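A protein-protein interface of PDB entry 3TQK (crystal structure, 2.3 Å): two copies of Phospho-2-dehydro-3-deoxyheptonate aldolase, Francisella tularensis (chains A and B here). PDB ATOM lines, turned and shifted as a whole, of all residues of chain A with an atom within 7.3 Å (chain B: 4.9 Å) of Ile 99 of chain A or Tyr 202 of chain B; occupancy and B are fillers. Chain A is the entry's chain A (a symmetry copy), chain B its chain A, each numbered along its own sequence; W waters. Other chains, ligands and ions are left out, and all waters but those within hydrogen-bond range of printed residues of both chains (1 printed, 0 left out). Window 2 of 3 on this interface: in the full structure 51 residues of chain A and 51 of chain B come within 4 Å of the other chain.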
ATOM      1  N   PRO A  95     -22.662  13.173   4.144  1.00  0.00           N
ATOM      2  CA  PRO A  95     -22.461  14.052   5.306  1.00  0.00           C
ATOM      3  C   PRO A  95     -23.742  14.305   6.102  1.00  0.00           C
ATOM      4  O   PRO A  95     -24.814  14.519   5.507  1.00  0.00           O
ATOM      5  CB  PRO A  95     -21.969  15.370   4.688  1.00  0.00           C
ATOM      6  CG  PRO A  95     -21.938  15.153   3.164  1.00  0.00           C
ATOM      7  CD  PRO A  95     -22.026  13.698   2.918  1.00  0.00           C
ATOM      8  N   ARG A  96     -23.615  14.293   7.432  1.00  0.00           N
ATOM      9  CA  ARG A  96     -24.725  14.571   8.355  1.00  0.00           C
ATOM     10  C   ARG A  96     -24.306  15.602   9.407  1.00  0.00           C
ATOM     11  O   ARG A  96     -23.213  15.503   9.968  1.00  0.00           O
ATOM     12  CB  ARG A  96     -25.159  13.293   9.078  1.00  0.00           C
ATOM     13  CG  ARG A  96     -25.564  12.133   8.169  1.00  0.00           C
ATOM     14  CD  ARG A  96     -26.890  12.393   7.435  1.00  0.00           C
ATOM     15  NE  ARG A  96     -27.227  11.295   6.522  1.00  0.00           N
ATOM     16  CZ  ARG A  96     -28.300  11.254   5.731  1.00  0.00           C
ATOM     17  NH1 ARG A  96     -29.174  12.255   5.715  1.00  0.00           N
ATOM     18  NH2 ARG A  96     -28.500  10.198   4.947  1.00  0.00           N
ATOM     19  N   THR A  97     -25.178  16.572   9.676  1.00  0.00           N
ATOM     20  CA  THR A  97     -24.923  17.618  10.669  1.00  0.00           C
ATOM     21  C   THR A  97     -24.555  17.028  12.039  1.00  0.00           C
ATOM     22  O   THR A  97     -23.613  17.493  12.681  1.00  0.00           O
ATOM     23  CB  THR A  97     -26.155  18.539  10.825  1.00  0.00           C
ATOM     24  OG1 THR A  97     -26.506  19.075   9.548  1.00  0.00           O
ATOM     25  CG2 THR A  97     -25.880  19.691  11.795  1.00  0.00           C
ATOM     26  N   THR A  98     -25.307  16.016  12.472  1.00  0.00           N
ATOM     27  CA  THR A  98     -24.975  15.256  13.671  1.00  0.00           C
ATOM     28  C   THR A  98     -25.043  13.746  13.394  1.00  0.00           C
ATOM     29  O   THR A  98     -24.005  13.085  13.296  1.00  0.00           O
ATOM     30  CB  THR A  98     -25.863  15.654  14.897  1.00  0.00           C
ATOM     31  OG1 THR A  98     -27.246  15.412  14.609  1.00  0.00           O
ATOM     32  CG2 THR A  98     -25.670  17.126  15.246  1.00  0.00           C
ATOM     33  N   ILE A  99     -26.254  13.208  13.252  1.00  0.00           N
ATOM     34  CA  ILE A  99     -26.434  11.771  13.028  1.00  0.00           C
ATOM     35  C   ILE A  99     -27.279  11.457  11.785  1.00  0.00           C
ATOM     36  O   ILE A  99     -27.798  12.362  11.128  1.00  0.00           O
ATOM     37  CB  ILE A  99     -27.029  11.077  14.285  1.00  0.00           C
ATOM     38  CG1 ILE A  99     -28.393  11.681  14.659  1.00  0.00           C
ATOM     39  CG2 ILE A  99     -26.033  11.174  15.441  1.00  0.00           C
ATOM     40  CD1 ILE A  99     -29.265  10.754  15.484  1.00  0.00           C
ATOM     41  N   GLY A 100     -27.388  10.164  11.473  1.00  0.00           N
ATOM     42  CA  GLY A 100     -28.123   9.685  10.292  1.00  0.00           C
ATOM     43  C   GLY A 100     -27.371   8.583   9.559  1.00  0.00           C
ATOM     44  O   GLY A 100     -26.200   8.333   9.848  1.00  0.00           O
ATOM     45  N   TRP A 101     -28.055   7.911   8.626  1.00  0.00           N
ATOM     46  CA  TRP A 101     -27.411   6.938   7.727  1.00  0.00           C
ATOM     47  C   TRP A 101     -26.169   7.566   7.147  1.00  0.00           C
ATOM     48  O   TRP A 101     -26.258   8.616   6.528  1.00  0.00           O
ATOM     49  CB  TRP A 101     -28.341   6.551   6.577  1.00  0.00           C
ATOM     50  CG  TRP A 101     -27.821   5.454   5.682  1.00  0.00           C
ATOM     51  CD1 TRP A 101     -27.568   4.165   6.034  1.00  0.00           C
ATOM     52  CD2 TRP A 101     -27.534   5.549   4.278  1.00  0.00           C
ATOM     53  NE1 TRP A 101     -27.123   3.448   4.941  1.00  0.00           N
ATOM     54  CE2 TRP A 101     -27.103   4.272   3.851  1.00  0.00           C
ATOM     55  CE3 TRP A 101     -27.595   6.587   3.343  1.00  0.00           C
ATOM     56  CZ2 TRP A 101     -26.732   4.009   2.528  1.00  0.00           C
ATOM     57  CZ3 TRP A 101     -27.238   6.319   2.025  1.00  0.00           C
ATOM     58  CH2 TRP A 101     -26.808   5.041   1.634  1.00  0.00           C
ATOM     59  N   LYS A 102     -25.024   6.921   7.360  1.00  0.00           N
ATOM     60  CA  LYS A 102     -23.734   7.438   6.901  1.00  0.00           C
ATOM     61  C   LYS A 102     -23.498   7.132   5.424  1.00  0.00           C
ATOM     62  O   LYS A 102     -22.677   7.792   4.785  1.00  0.00           O
ATOM     63  CB  LYS A 102     -22.569   6.831   7.704  1.00  0.00           C
ATOM     64  CG  LYS A 102     -21.930   7.724   8.768  1.00  0.00           C
ATOM     65  CD  LYS A 102     -22.442   7.435  10.195  1.00  0.00           C
ATOM     66  CE  LYS A 102     -21.284   7.471  11.203  1.00  0.00           C
ATOM     67  NZ  LYS A 102     -21.615   6.944  12.541  1.00  0.00           N
ATOM     68  N   SER B 174     -16.127   9.908  20.207  1.00  0.00           N
ATOM     69  CA  SER B 174     -17.196   9.101  20.804  1.00  0.00           C
ATOM     70  C   SER B 174     -16.693   7.785  21.403  1.00  0.00           C
ATOM     71  O   SER B 174     -17.427   7.127  22.141  1.00  0.00           O
ATOM     72  CB  SER B 174     -18.291   8.789  19.776  1.00  0.00           C
ATOM     73  OG  SER B 174     -17.891   7.747  18.890  1.00  0.00           O
ATOM     74  N   LYS B 198     -22.547  17.156  20.142  1.00  0.00           N
ATOM     75  CA  LYS B 198     -23.771  16.385  20.068  1.00  0.00           C
ATOM     76  C   LYS B 198     -23.539  15.029  19.407  1.00  0.00           C
ATOM     77  O   LYS B 198     -23.928  13.991  19.956  1.00  0.00           O
ATOM     78  CB  LYS B 198     -24.830  17.159  19.287  1.00  0.00           C
ATOM     79  CG  LYS B 198     -26.202  16.490  19.198  1.00  0.00           C
ATOM     80  CD  LYS B 198     -26.780  16.195  20.567  1.00  0.00           C
ATOM     81  CE  LYS B 198     -28.279  15.865  20.497  1.00  0.00           C
ATOM     82  NZ  LYS B 198     -28.738  15.380  21.829  1.00  0.00           N
ATOM     83  N   SER B 199     -22.902  15.047  18.242  1.00  0.00           N
ATOM     84  CA  SER B 199     -22.601  13.828  17.506  1.00  0.00           C
ATOM     85  C   SER B 199     -21.762  12.859  18.318  1.00  0.00           C
ATOM     86  O   SER B 199     -21.983  11.656  18.264  1.00  0.00           O
ATOM     87  CB  SER B 199     -21.893  14.152  16.194  1.00  0.00           C
ATOM     88  OG  SER B 199     -21.562  12.974  15.489  1.00  0.00           O
ATOM     89  N   ALA B 200     -20.808  13.387  19.072  1.00  0.00           N
ATOM     90  CA  ALA B 200     -19.888  12.570  19.862  1.00  0.00           C
ATOM     91  C   ALA B 200     -20.556  11.852  21.050  1.00  0.00           C
ATOM     92  O   ALA B 200     -19.999  10.876  21.577  1.00  0.00           O
ATOM     93  CB  ALA B 200     -18.700  13.423  20.344  1.00  0.00           C
ATOM     94  N   THR B 201     -21.726  12.329  21.479  1.00  0.00           N
ATOM     95  CA  THR B 201     -22.494  11.640  22.526  1.00  0.00           C
ATOM     96  C   THR B 201     -23.105  10.315  22.039  1.00  0.00           C
ATOM     97  O   THR B 201     -23.465   9.475  22.866  1.00  0.00           O
ATOM     98  CB  THR B 201     -23.674  12.496  23.108  1.00  0.00           C
ATOM     99  OG1 THR B 201     -24.632  12.780  22.078  1.00  0.00           O
ATOM    100  CG2 THR B 201     -23.181  13.794  23.751  1.00  0.00           C
ATOM    101  N   TYR B 202     -23.234  10.128  20.722  1.00  0.00           N
ATOM    102  CA  TYR B 202     -23.866   8.933  20.177  1.00  0.00           C
ATOM    103  C   TYR B 202     -22.918   7.771  19.993  1.00  0.00           C
ATOM    104  O   TYR B 202     -21.712   7.967  19.882  1.00  0.00           O
ATOM    105  CB  TYR B 202     -24.513   9.240  18.834  1.00  0.00           C
ATOM    106  CG  TYR B 202     -25.756  10.096  18.957  1.00  0.00           C
ATOM    107  CD1 TYR B 202     -27.000   9.526  19.195  1.00  0.00           C
ATOM    108  CD2 TYR B 202     -25.679  11.472  18.834  1.00  0.00           C
ATOM    109  CE1 TYR B 202     -28.150  10.323  19.299  1.00  0.00           C
ATOM    110  CE2 TYR B 202     -26.790  12.265  18.935  1.00  0.00           C
ATOM    111  CZ  TYR B 202     -28.020  11.697  19.169  1.00  0.00           C
ATOM    112  OH  TYR B 202     -29.102  12.522  19.266  1.00  0.00           O
ATOM    113  N   PRO B 203     -23.460   6.544  19.944  1.00  0.00           N
ATOM    114  CA  PRO B 203     -22.634   5.418  19.556  1.00  0.00           C
ATOM    115  C   PRO B 203     -22.388   5.468  18.049  1.00  0.00           C
ATOM    116  O   PRO B 203     -23.252   5.911  17.282  1.00  0.00           O
ATOM    117  CB  PRO B 203     -23.474   4.184  19.950  1.00  0.00           C
ATOM    118  CG  PRO B 203     -24.721   4.717  20.626  1.00  0.00           C
ATOM    119  CD  PRO B 203     -24.854   6.140  20.204  1.00  0.00           C
ATOM    120  N   HIS B 204     -21.212   5.032  17.637  1.00  0.00           N
ATOM    121  CA  HIS B 204     -20.837   5.029  16.237  1.00  0.00           C
ATOM    122  C   HIS B 204     -20.131   3.710  15.914  1.00  0.00           C
ATOM    123  O   HIS B 204     -19.481   3.112  16.782  1.00  0.00           O
ATOM    124  CB  HIS B 204     -19.876   6.202  15.944  1.00  0.00           C
ATOM    125  CG  HIS B 204     -20.523   7.551  15.987  1.00  0.00           C
ATOM    126  ND1 HIS B 204     -21.193   8.086  14.911  1.00  0.00           N
ATOM    127  CD2 HIS B 204     -20.615   8.469  16.980  1.00  0.00           C
ATOM    128  CE1 HIS B 204     -21.665   9.280  15.236  1.00  0.00           C
ATOM    129  NE2 HIS B 204     -21.313   9.544  16.483  1.00  0.00           N
ATOM    130  N   THR B 220     -18.520   2.206  19.203  1.00  0.00           N
ATOM    131  CA  THR B 220     -18.344   3.048  20.371  1.00  0.00           C
ATOM    132  C   THR B 220     -19.623   3.191  21.169  1.00  0.00           C
ATOM    133  O   THR B 220     -20.710   2.862  20.691  1.00  0.00           O
ATOM    134  CB  THR B 220     -17.845   4.452  19.995  1.00  0.00           C
ATOM    135  OG1 THR B 220     -18.888   5.185  19.344  1.00  0.00           O
ATOM    136  CG2 THR B 220     -16.620   4.369  19.103  1.00  0.00           C
ATOM    137  N   LYS B 221     -19.464   3.708  22.385  1.00  0.00           N
ATOM    138  CA  LYS B 221     -20.554   3.932  23.337  1.00  0.00           C
ATOM    139  C   LYS B 221     -21.076   5.357  23.329  1.00  0.00           C
ATOM    140  O   LYS B 221     -22.173   5.620  23.824  1.00  0.00           O
ATOM    141  CB  LYS B 221     -20.067   3.599  24.756  1.00  0.00           C
ATOM    142  CG  LYS B 221     -20.318   2.141  25.146  1.00  0.00           C
ATOM    143  CD  LYS B 221     -19.111   1.462  25.805  1.00  0.00           C
ATOM    144  CE  LYS B 221     -19.014   1.735  27.296  1.00  0.00           C
ATOM    145  NZ  LYS B 221     -18.144   0.707  27.972  1.00  0.00           N
ATOM    146  N   GLY B 222     -20.277   6.273  22.798  1.00  0.00           N
ATOM    147  CA  GLY B 222     -20.545   7.703  22.894  1.00  0.00           C
ATOM    148  C   GLY B 222     -19.780   8.298  24.057  1.00  0.00           C
ATOM    149  O   GLY B 222     -19.428   7.590  24.993  1.00  0.00           O
HETATM  150  O   HOH W   1     -21.588  14.316  12.310  1.00  0.00           O
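OG of Ser 199 of chain B lies within hydrogen-bond range of O of Thr 98 of chain A, 3.3 Å away. A ring nitrogen (ND1) of His 204 of chain B lies within hydrogen-bond range of the side-chain amino group of Lys 102 of chain A, at 2.7 Å.
Water W1 lies within hydrogen-bond range of the backbone carbonyl oxygen (O) of Thr 98 of chain A, the backbone carbonyl oxygen (O) of Arg 96 of chain A and the side-chain hydroxyl (OG) of Ser 199 of chain B.
O of Ser 199 of chain B lies within hydrogen-bond range of NE2 of His 204 of chain B, 2.8 Å away. N of Thr 220 of chain B sits at hydrogen-bond distance from O of His 204 of chain B (2.8 Å).
No position is printed for both chains.
Among the printed residues, merely in contact across the chains: Ile 99 of chain A with Tyr 202 of chain B (3.4 Å).
Of chain B, only Tyr 202 comes within 4 Å of Ile 99 of chain A. Of chain A, only Ile 99 (3.4 Å) comes within 4 Å of Tyr 202 of chain B. Printed residues of chain B within 4 Å of Thr 98 of chain A: Ser 199. Printed residues of chain A within 4 Å of His 204 of chain B: Lys 102 (2.7 Å). Of the printed residues of chain A, Ser 199 of chain B touches Thr 98 (3.3 Å). Pro 203 of chain B touches none of the printed residues of chain A. Arg 96 of chain A touches none of the printed residues of chain B. The nearest printed residue of chain B that does not touch Thr 98 of chain A is Lys 198 of chain B (4.04 Å).
Printed residues of chain A that touch a printed residue of chain B: Thr 98, Ile 99 and Lys 102. Of the 11 printed residues of chain B, 3 touch a printed residue of chain A. Printed residues of chain B that touch a printed residue of chain A: Ser 199, Tyr 202 and His 204. Hydrophobic or aromatic side chains of chain B that line the printed part of chain A: Tyr 202 and His 204. Along chain B the printed residues that touch a printed residue of chain A span positions 199 to 204. Among the printed residues, 3 pairs touch across the chains. Among the printed residues, no Asp or Glu carboxylate lies within 4 Å of a Lys or Arg side-chain nitrogen of the other chain.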
